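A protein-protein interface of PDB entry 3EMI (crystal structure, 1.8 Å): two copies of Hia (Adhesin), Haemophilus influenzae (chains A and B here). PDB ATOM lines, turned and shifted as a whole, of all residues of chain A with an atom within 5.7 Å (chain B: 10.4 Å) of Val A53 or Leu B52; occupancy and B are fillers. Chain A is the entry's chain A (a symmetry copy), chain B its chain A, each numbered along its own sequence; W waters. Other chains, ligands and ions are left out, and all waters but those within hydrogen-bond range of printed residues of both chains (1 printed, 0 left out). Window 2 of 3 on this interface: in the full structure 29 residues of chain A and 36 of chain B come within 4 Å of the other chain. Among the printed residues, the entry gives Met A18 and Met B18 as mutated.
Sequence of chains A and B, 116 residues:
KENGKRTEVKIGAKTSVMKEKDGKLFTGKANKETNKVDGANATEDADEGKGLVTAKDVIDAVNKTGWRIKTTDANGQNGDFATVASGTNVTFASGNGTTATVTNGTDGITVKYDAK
Water W1 lies within hydrogen-bond range of the backbone carbonyl oxygen of Val A53 and the backbone NH of Val B53.
Thr A54 touches Gly B51, but with the chains exchanged Gly A51 does not touch Thr B54 (11.8 Å).
Ala A55 touches Ser B16, but with the chains exchanged Ser A16 does not touch Ala B55 (14.9 Å).
Ala A55 touches Gly B51, but with the chains exchanged Gly A51 does not touch Ala B55 (11.8 Å).
Ala A55 touches Val B53, but with the chains exchanged Val A53 does not touch Ala B55 (9.0 Å).
Of the 10 pairs that touch across the chains among the printed residues, none has its exchanged pair printed and touching as well.
O of Gly B49 sits at hydrogen-bond distance from N of Ala A55.
O of Gly B51 lies within hydrogen-bond range of N of Ala A55, 2.9 Å away.
OD1 of Asp B47 sits at hydrogen-bond distance from OG of Ser B16 (2.9 Å).
The backbone NH (N) of Ser B16 is in hydrogen-bond range of the backbone carbonyl oxygen (O) of Leu B52 (2.9 Å).
OG of Ser B16 lies within hydrogen-bond range of N of Lys B50 (3.4 Å).
OG of Ser B16 sits at hydrogen-bond distance from N of Gly B51, 2.7 Å away.
The side-chain amino group (NZ) of Lys B50 lies within salt-bridge range of the side-chain carboxylate (OE1) of Glu B48 (2.7 Å).
The backbone carbonyl oxygen of Lys B14 lies within hydrogen-bond range of the backbone NH of Leu B52 (3.0 Å).
Hydrophobic or aromatic side chains of chain A within 4 Å of the printed part of chain B: Ala A55 and Val A58.
Printed residues of chain B that touch a printed residue of chain A: Ser B16, Met B18, Gly B49, Lys B50, Gly B51, Leu B52 and Val B53.
Along chain B the printed residues that touch a printed residue of chain A span positions 16 to 53.
Among the printed residues, no Asp or Glu carboxylate lies within 4 Å of a Lys or Arg side-chain nitrogen of the other chain.
Leu B52 touches one residue of chain A.
No residue of chain B comes within 4 Å of Leu A52.
No residue of chain B comes within 4 Å of Asp A57.
Of the printed residues of chain A, Lys B50 touches Thr A54 (3.6 Å).
Of the printed residues of chain B, Ala A55 touches Ser B16, Met B18, Gly B49, Gly B51 and Val B53.
Glu B48 touches none of the printed residues of chain A.
The nearest residue of chain B that does not touch Val A53 is Gly B51 (4.5 Å).
The nearest residue of chain A that does not touch Leu B52 is Leu A52 (4.2 Å).
The nearest printed residue of chain A that does not touch Lys B50 is Ala A55 (5.0 Å).
Leu B52 touches Val A53.
Gly B49 touches Thr A54 (O to CB, 3.3 Å).
CG2 of Thr A54 touches O of Lys B50, at 3.6 Å.
Thr A54 touches Gly B51.
CB of Ser B16 touches CB of Ala A55 (3.4 Å).
CG of Met B18 touches CB of Ala A55, at 3.98 Å.
Ala A55 touches Val B53.
Val A58 touches Met B18.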
ATOM      1  N   THR A  15      23.938 -14.404  20.842  1.00  0.00           N
ATOM      2  CA  THR A  15      24.983 -13.669  21.532  1.00  0.00           C
ATOM      3  C   THR A  15      26.339 -14.306  21.252  1.00  0.00           C
ATOM      4  O   THR A  15      26.425 -15.470  20.850  1.00  0.00           O
ATOM      5  CB  THR A  15      24.745 -13.630  23.056  1.00  0.00           C
ATOM      6  OG1 THR A  15      24.691 -14.968  23.568  1.00  0.00           O
ATOM      7  CG2 THR A  15      23.448 -12.912  23.376  1.00  0.00           C
ATOM      8  N   SER A  16      27.390 -13.526  21.453  1.00  0.00           N
ATOM      9  CA  SER A  16      28.748 -14.022  21.332  1.00  0.00           C
ATOM     10  C   SER A  16      29.406 -13.909  22.689  1.00  0.00           C
ATOM     11  O   SER A  16      29.045 -13.052  23.483  1.00  0.00           O
ATOM     12  CB  SER A  16      29.533 -13.201  20.315  1.00  0.00           C
ATOM     13  OG  SER A  16      29.311 -13.664  18.999  1.00  0.00           O
ATOM     14  N   MET A  18      32.718 -13.313  25.264  1.00  0.00           N
ATOM     15  CA  MET A  18      33.930 -12.511  25.321  1.00  0.00           C
ATOM     16  C   MET A  18      34.862 -13.206  26.293  1.00  0.00           C
ATOM     17  O   MET A  18      34.504 -13.427  27.460  1.00  0.00           O
ATOM     18  CB  MET A  18      33.618 -11.075  25.767  1.00  0.00           C
ATOM     19  CG  MET A  18      32.853 -10.258  24.712  1.00  0.00           C
ATOM     20  SD  MET A  18      32.438  -8.566  25.216  1.00  0.00           S
ATOM     21  CE  MET A  18      31.241  -8.900  26.501  1.00  0.00           C
ATOM     22  N   GLY A  51      28.121 -11.872  17.370  1.00  0.00           N
ATOM     23  CA  GLY A  51      26.894 -11.838  18.142  1.00  0.00           C
ATOM     24  C   GLY A  51      26.753 -10.649  19.079  1.00  0.00           C
ATOM     25  O   GLY A  51      27.705  -9.900  19.325  1.00  0.00           O
ATOM     26  N   LEU A  52      25.546 -10.481  19.605  1.00  0.00           N
ATOM     27  CA  LEU A  52      25.275  -9.436  20.579  1.00  0.00           C
ATOM     28  C   LEU A  52      25.813  -9.830  21.948  1.00  0.00           C
ATOM     29  O   LEU A  52      26.217 -10.973  22.158  1.00  0.00           O
ATOM     30  CB  LEU A  52      23.773  -9.185  20.664  1.00  0.00           C
ATOM     31  CG  LEU A  52      23.143  -8.663  19.374  1.00  0.00           C
ATOM     32  CD1 LEU A  52      21.646  -8.614  19.522  1.00  0.00           C
ATOM     33  CD2 LEU A  52      23.707  -7.293  19.029  1.00  0.00           C
ATOM     34  N   VAL A  53      25.812  -8.882  22.880  1.00  0.00           N
ATOM     35  CA  VAL A  53      26.218  -9.151  24.253  1.00  0.00           C
ATOM     36  C   VAL A  53      25.205  -8.504  25.203  1.00  0.00           C
ATOM     37  O   VAL A  53      24.464  -7.607  24.805  1.00  0.00           O
ATOM     38  CB  VAL A  53      27.634  -8.600  24.538  1.00  0.00           C
ATOM     39  CG1 VAL A  53      28.641  -9.167  23.536  1.00  0.00           C
ATOM     40  CG2 VAL A  53      27.640  -7.077  24.481  1.00  0.00           C
ATOM     41  N   THR A  54      25.160  -8.973  26.450  1.00  0.00           N
ATOM     42  CA  THR A  54      24.291  -8.367  27.453  1.00  0.00           C
ATOM     43  C   THR A  54      25.079  -7.394  28.321  1.00  0.00           C
ATOM     44  O   THR A  54      26.311  -7.388  28.302  1.00  0.00           O
ATOM     45  CB  THR A  54      23.659  -9.419  28.394  1.00  0.00           C
ATOM     46  OG1 THR A  54      24.688 -10.057  29.163  1.00  0.00           O
ATOM     47  CG2 THR A  54      22.899 -10.474  27.599  1.00  0.00           C
ATOM     48  N   ALA A  55      24.368  -6.579  29.097  1.00  0.00           N
ATOM     49  CA  ALA A  55      25.019  -5.708  30.077  1.00  0.00           C
ATOM     50  C   ALA A  55      25.914  -6.520  31.012  1.00  0.00           C
ATOM     51  O   ALA A  55      27.074  -6.156  31.256  1.00  0.00           O
ATOM     52  CB  ALA A  55      23.983  -4.952  30.878  1.00  0.00           C
ATOM     53  N   ASP A  57      27.298  -9.366  30.517  1.00  0.00           N
ATOM     54  CA  ASP A  57      28.456  -9.848  29.767  1.00  0.00           C
ATOM     55  C   ASP A  57      29.547  -8.777  29.756  1.00  0.00           C
ATOM     56  O   ASP A  57      30.717  -9.057  30.012  1.00  0.00           O
ATOM     57  CB  ASP A  57      28.085 -10.175  28.322  1.00  0.00           C
ATOM     58  CG  ASP A  57      27.183 -11.392  28.195  1.00  0.00           C
ATOM     59  OD1 ASP A  57      27.085 -12.184  29.160  1.00  0.00           O
ATOM     60  OD2 ASP A  57      26.577 -11.549  27.112  1.00  0.00           O
ATOM     61  N   VAL A  58      29.158  -7.548  29.425  1.00  0.00           N
ATOM     62  CA  VAL A  58      30.117  -6.452  29.306  1.00  0.00           C
ATOM     63  C   VAL A  58      30.712  -6.107  30.665  1.00  0.00           C
ATOM     64  O   VAL A  58      31.928  -5.934  30.804  1.00  0.00           O
ATOM     65  CB  VAL A  58      29.462  -5.205  28.696  1.00  0.00           C
ATOM     66  CG1 VAL A  58      30.435  -4.029  28.702  1.00  0.00           C
ATOM     67  CG2 VAL A  58      28.993  -5.506  27.277  1.00  0.00           C
ATOM     68  N   ILE B  11      10.209  -2.808  16.981  1.00  0.00           N
ATOM     69  CA  ILE B  11      10.325  -3.895  17.942  1.00  0.00           C
ATOM     70  C   ILE B  11      11.300  -3.514  19.049  1.00  0.00           C
ATOM     71  O   ILE B  11      12.507  -3.460  18.829  1.00  0.00           O
ATOM     72  CB  ILE B  11      10.790  -5.194  17.263  1.00  0.00           C
ATOM     73  CG1 ILE B  11       9.828  -5.565  16.131  1.00  0.00           C
ATOM     74  CG2 ILE B  11      10.888  -6.326  18.273  1.00  0.00           C
ATOM     75  CD1 ILE B  11      10.274  -6.751  15.318  1.00  0.00           C
ATOM     76  N   GLY B  12      10.768  -3.248  20.236  1.00  0.00           N
ATOM     77  CA  GLY B  12      11.578  -2.802  21.355  1.00  0.00           C
ATOM     78  C   GLY B  12      12.398  -3.906  21.996  1.00  0.00           C
ATOM     79  O   GLY B  12      11.887  -4.985  22.304  1.00  0.00           O
ATOM     80  N   ALA B  13      13.682  -3.635  22.187  1.00  0.00           N
ATOM     81  CA  ALA B  13      14.559  -4.552  22.892  1.00  0.00           C
ATOM     82  C   ALA B  13      14.978  -3.874  24.184  1.00  0.00           C
ATOM     83  O   ALA B  13      15.554  -2.788  24.165  1.00  0.00           O
ATOM     84  CB  ALA B  13      15.775  -4.896  22.044  1.00  0.00           C
ATOM     85  N   LYS B  14      14.667  -4.503  25.307  1.00  0.00           N
ATOM     86  CA  LYS B  14      14.967  -3.902  26.597  1.00  0.00           C
ATOM     87  C   LYS B  14      16.471  -3.789  26.813  1.00  0.00           C
ATOM     88  O   LYS B  14      17.218  -4.725  26.517  1.00  0.00           O
ATOM     89  CB  LYS B  14      14.334  -4.706  27.717  1.00  0.00           C
ATOM     90  N   THR B  15      16.906  -2.641  27.322  1.00  0.00           N
ATOM     91  CA  THR B  15      18.304  -2.454  27.665  1.00  0.00           C
ATOM     92  C   THR B  15      18.496  -2.607  29.168  1.00  0.00           C
ATOM     93  O   THR B  15      17.543  -2.494  29.947  1.00  0.00           O
ATOM     94  CB  THR B  15      18.822  -1.068  27.225  1.00  0.00           C
ATOM     95  OG1 THR B  15      18.039  -0.042  27.852  1.00  0.00           O
ATOM     96  CG2 THR B  15      18.738  -0.919  25.718  1.00  0.00           C
ATOM     97  N   SER B  16      19.731  -2.880  29.564  1.00  0.00           N
ATOM     98  CA  SER B  16      20.089  -2.948  30.967  1.00  0.00           C
ATOM     99  C   SER B  16      21.095  -1.854  31.243  1.00  0.00           C
ATOM    100  O   SER B  16      21.832  -1.452  30.355  1.00  0.00           O
ATOM    101  CB  SER B  16      20.704  -4.302  31.301  1.00  0.00           C
ATOM    102  OG  SER B  16      19.710  -5.269  31.570  1.00  0.00           O
ATOM    103  N   VAL B  17      21.112  -1.365  32.476  1.00  0.00           N
ATOM    104  CA  VAL B  17      22.049  -0.325  32.870  1.00  0.00           C
ATOM    105  C   VAL B  17      23.362  -0.960  33.303  1.00  0.00           C
ATOM    106  O   VAL B  17      23.402  -2.132  33.668  1.00  0.00           O
ATOM    107  CB  VAL B  17      21.464   0.531  34.029  1.00  0.00           C
ATOM    108  CG1 VAL B  17      21.342  -0.308  35.301  1.00  0.00           C
ATOM    109  CG2 VAL B  17      22.305   1.778  34.281  1.00  0.00           C
ATOM    110  N   MET B  18      24.440  -0.189  33.241  1.00  0.00           N
ATOM    111  CA  MET B  18      25.722  -0.620  33.776  1.00  0.00           C
ATOM    112  C   MET B  18      26.146   0.431  34.783  1.00  0.00           C
ATOM    113  O   MET B  18      26.262   1.617  34.443  1.00  0.00           O
ATOM    114  CB  MET B  18      26.760  -0.778  32.656  1.00  0.00           C
ATOM    115  CG  MET B  18      26.486  -1.975  31.730  1.00  0.00           C
ATOM    116  SD  MET B  18      27.673  -2.176  30.375  1.00  0.00           S
ATOM    117  CE  MET B  18      27.284  -0.732  29.394  1.00  0.00           C
ATOM    118  N   ASP B  47      17.675  -4.673  38.179  1.00  0.00           N
ATOM    119  CA  ASP B  47      18.294  -4.978  36.885  1.00  0.00           C
ATOM    120  C   ASP B  47      19.471  -5.946  37.002  1.00  0.00           C
ATOM    121  O   ASP B  47      20.514  -5.591  37.555  1.00  0.00           O
ATOM    122  CB  ASP B  47      18.767  -3.678  36.235  1.00  0.00           C
ATOM    123  CG  ASP B  47      19.176  -3.854  34.789  1.00  0.00           C
ATOM    124  OD1 ASP B  47      19.659  -4.942  34.418  1.00  0.00           O
ATOM    125  OD2 ASP B  47      19.023  -2.886  34.016  1.00  0.00           O
ATOM    126  N   GLU B  48      19.310  -7.152  36.465  1.00  0.00           N
ATOM    127  CA  GLU B  48      20.350  -8.178  36.566  1.00  0.00           C
ATOM    128  C   GLU B  48      21.277  -8.213  35.350  1.00  0.00           C
ATOM    129  O   GLU B  48      22.125  -9.103  35.227  1.00  0.00           O
ATOM    130  CB  GLU B  48      19.732  -9.557  36.821  1.00  0.00           C
ATOM    131  CG  GLU B  48      18.881  -9.591  38.083  1.00  0.00           C
ATOM    132  CD  GLU B  48      18.514 -10.990  38.524  1.00  0.00           C
ATOM    133  OE1 GLU B  48      18.577 -11.921  37.695  1.00  0.00           O
ATOM    134  OE2 GLU B  48      18.153 -11.152  39.707  1.00  0.00           O
ATOM    135  N   GLY B  49      21.112  -7.239  34.457  1.00  0.00           N
ATOM    136  CA  GLY B  49      22.000  -7.083  33.320  1.00  0.00           C
ATOM    137  C   GLY B  49      21.709  -8.005  32.150  1.00  0.00           C
ATOM    138  O   GLY B  49      22.576  -8.232  31.305  1.00  0.00           O
ATOM    139  N   LYS B  50      20.487  -8.522  32.082  1.00  0.00           N
ATOM    140  CA  LYS B  50      20.109  -9.421  30.994  1.00  0.00           C
ATOM    141  C   LYS B  50      19.806  -8.652  29.715  1.00  0.00           C
ATOM    142  O   LYS B  50      19.714  -9.238  28.642  1.00  0.00           O
ATOM    143  CB  LYS B  50      18.898 -10.272  31.377  1.00  0.00           C
ATOM    144  CG  LYS B  50      19.167 -11.296  32.466  1.00  0.00           C
ATOM    145  CD  LYS B  50      17.972 -12.232  32.627  1.00  0.00           C
ATOM    146  CE  LYS B  50      18.168 -13.186  33.800  1.00  0.00           C
ATOM    147  NZ  LYS B  50      18.191 -12.454  35.099  1.00  0.00           N
ATOM    148  N   GLY B  51      19.661  -7.337  29.837  1.00  0.00           N
ATOM    149  CA  GLY B  51      19.310  -6.505  28.703  1.00  0.00           C
ATOM    150  C   GLY B  51      20.467  -6.139  27.787  1.00  0.00           C
ATOM    151  O   GLY B  51      21.642  -6.347  28.112  1.00  0.00           O
ATOM    152  N   LEU B  52      20.123  -5.587  26.630  1.00  0.00           N
ATOM    153  CA  LEU B  52      21.119  -5.111  25.683  1.00  0.00           C
ATOM    154  C   LEU B  52      21.699  -3.780  26.143  1.00  0.00           C
ATOM    155  O   LEU B  52      21.191  -3.164  27.079  1.00  0.00           O
ATOM    156  CB  LEU B  52      20.488  -4.955  24.303  1.00  0.00           C
ATOM    157  CG  LEU B  52      19.982  -6.257  23.686  1.00  0.00           C
ATOM    158  CD1 LEU B  52      19.235  -5.961  22.414  1.00  0.00           C
ATOM    159  CD2 LEU B  52      21.142  -7.208  23.435  1.00  0.00           C
ATOM    160  N   VAL B  53      22.761  -3.335  25.476  1.00  0.00           N
ATOM    161  CA  VAL B  53      23.357  -2.036  25.757  1.00  0.00           C
ATOM    162  C   VAL B  53      23.639  -1.325  24.430  1.00  0.00           C
ATOM    163  O   VAL B  53      23.704  -1.966  23.382  1.00  0.00           O
ATOM    164  CB  VAL B  53      24.666  -2.183  26.566  1.00  0.00           C
ATOM    165  CG1 VAL B  53      24.416  -2.971  27.852  1.00  0.00           C
ATOM    166  CG2 VAL B  53      25.740  -2.868  25.730  1.00  0.00           C
ATOM    167  N   THR B  54      23.787  -0.002  24.472  1.00  0.00           N
ATOM    168  CA  THR B  54      24.144   0.757  23.277  1.00  0.00           C
ATOM    169  C   THR B  54      25.641   1.036  23.252  1.00  0.00           C
ATOM    170  O   THR B  54      26.331   0.866  24.258  1.00  0.00           O
ATOM    171  CB  THR B  54      23.416   2.120  23.209  1.00  0.00           C
ATOM    172  OG1 THR B  54      23.852   2.952  24.292  1.00  0.00           O
ATOM    173  CG2 THR B  54      21.906   1.937  23.293  1.00  0.00           C
ATOM    174  N   ALA B  55      26.143   1.484  22.102  1.00  0.00           N
ATOM    175  CA  ALA B  55      27.536   1.922  22.006  1.00  0.00           C
ATOM    176  C   ALA B  55      27.838   2.994  23.053  1.00  0.00           C
ATOM    177  O   ALA B  55      28.853   2.920  23.762  1.00  0.00           O
ATOM    178  CB  ALA B  55      27.822   2.457  20.620  1.00  0.00           C
ATOM    179  N   LYS B  56      26.979   4.009  23.142  1.00  0.00           N
ATOM    180  CA  LYS B  56      27.209   5.072  24.119  1.00  0.00           C
ATOM    181  C   LYS B  56      27.252   4.519  25.547  1.00  0.00           C
ATOM    182  O   LYS B  56      28.065   4.963  26.376  1.00  0.00           O
ATOM    183  CB  LYS B  56      26.152   6.170  24.007  1.00  0.00           C
ATOM    184  CG  LYS B  56      26.193   7.171  25.160  1.00  0.00           C
ATOM    185  CD  LYS B  56      25.059   8.164  25.060  1.00  0.00           C
ATOM    186  CE  LYS B  56      24.920   8.978  26.338  1.00  0.00           C
ATOM    187  NZ  LYS B  56      26.239   9.493  26.819  1.00  0.00           N
ATOM    188  N   ASP B  57      26.372   3.563  25.843  1.00  0.00           N
ATOM    189  CA  ASP B  57      26.371   2.947  27.167  1.00  0.00           C
ATOM    190  C   ASP B  57      27.749   2.356  27.464  1.00  0.00           C
ATOM    191  O   ASP B  57      28.312   2.561  28.539  1.00  0.00           O
ATOM    192  CB  ASP B  57      25.336   1.826  27.258  1.00  0.00           C
ATOM    193  CG  ASP B  57      23.903   2.330  27.218  1.00  0.00           C
ATOM    194  OD1 ASP B  57      23.673   3.541  27.438  1.00  0.00           O
ATOM    195  OD2 ASP B  57      23.006   1.494  26.969  1.00  0.00           O
ATOM    196  N   VAL B  58      28.277   1.594  26.510  1.00  0.00           N
ATOM    197  CA  VAL B  58      29.557   0.913  26.699  1.00  0.00           C
ATOM    198  C   VAL B  58      30.695   1.921  26.794  1.00  0.00           C
ATOM    199  O   VAL B  58      31.560   1.825  27.672  1.00  0.00           O
ATOM    200  CB  VAL B  58      29.834  -0.076  25.559  1.00  0.00           C
ATOM    201  CG1 VAL B  58      31.229  -0.679  25.697  1.00  0.00           C
ATOM    202  CG2 VAL B  58      28.774  -1.171  25.551  1.00  0.00           C
ATOM    203  N   VAL B  62      32.794   2.058  30.167  1.00  0.00           N
ATOM    204  CA  VAL B  62      34.206   1.697  30.075  1.00  0.00           C
ATOM    205  C   VAL B  62      35.102   2.864  30.479  1.00  0.00           C
ATOM    206  O   VAL B  62      36.125   2.677  31.146  1.00  0.00           O
ATOM    207  CB  VAL B  62      34.577   1.215  28.667  1.00  0.00           C
ATOM    208  CG1 VAL B  62      36.088   1.110  28.523  1.00  0.00           C
ATOM    209  CG2 VAL B  62      33.931  -0.141  28.405  1.00  0.00           C
HETATM  210  O   HOH W   1      24.001  -5.337  23.779  1.00  0.00           O
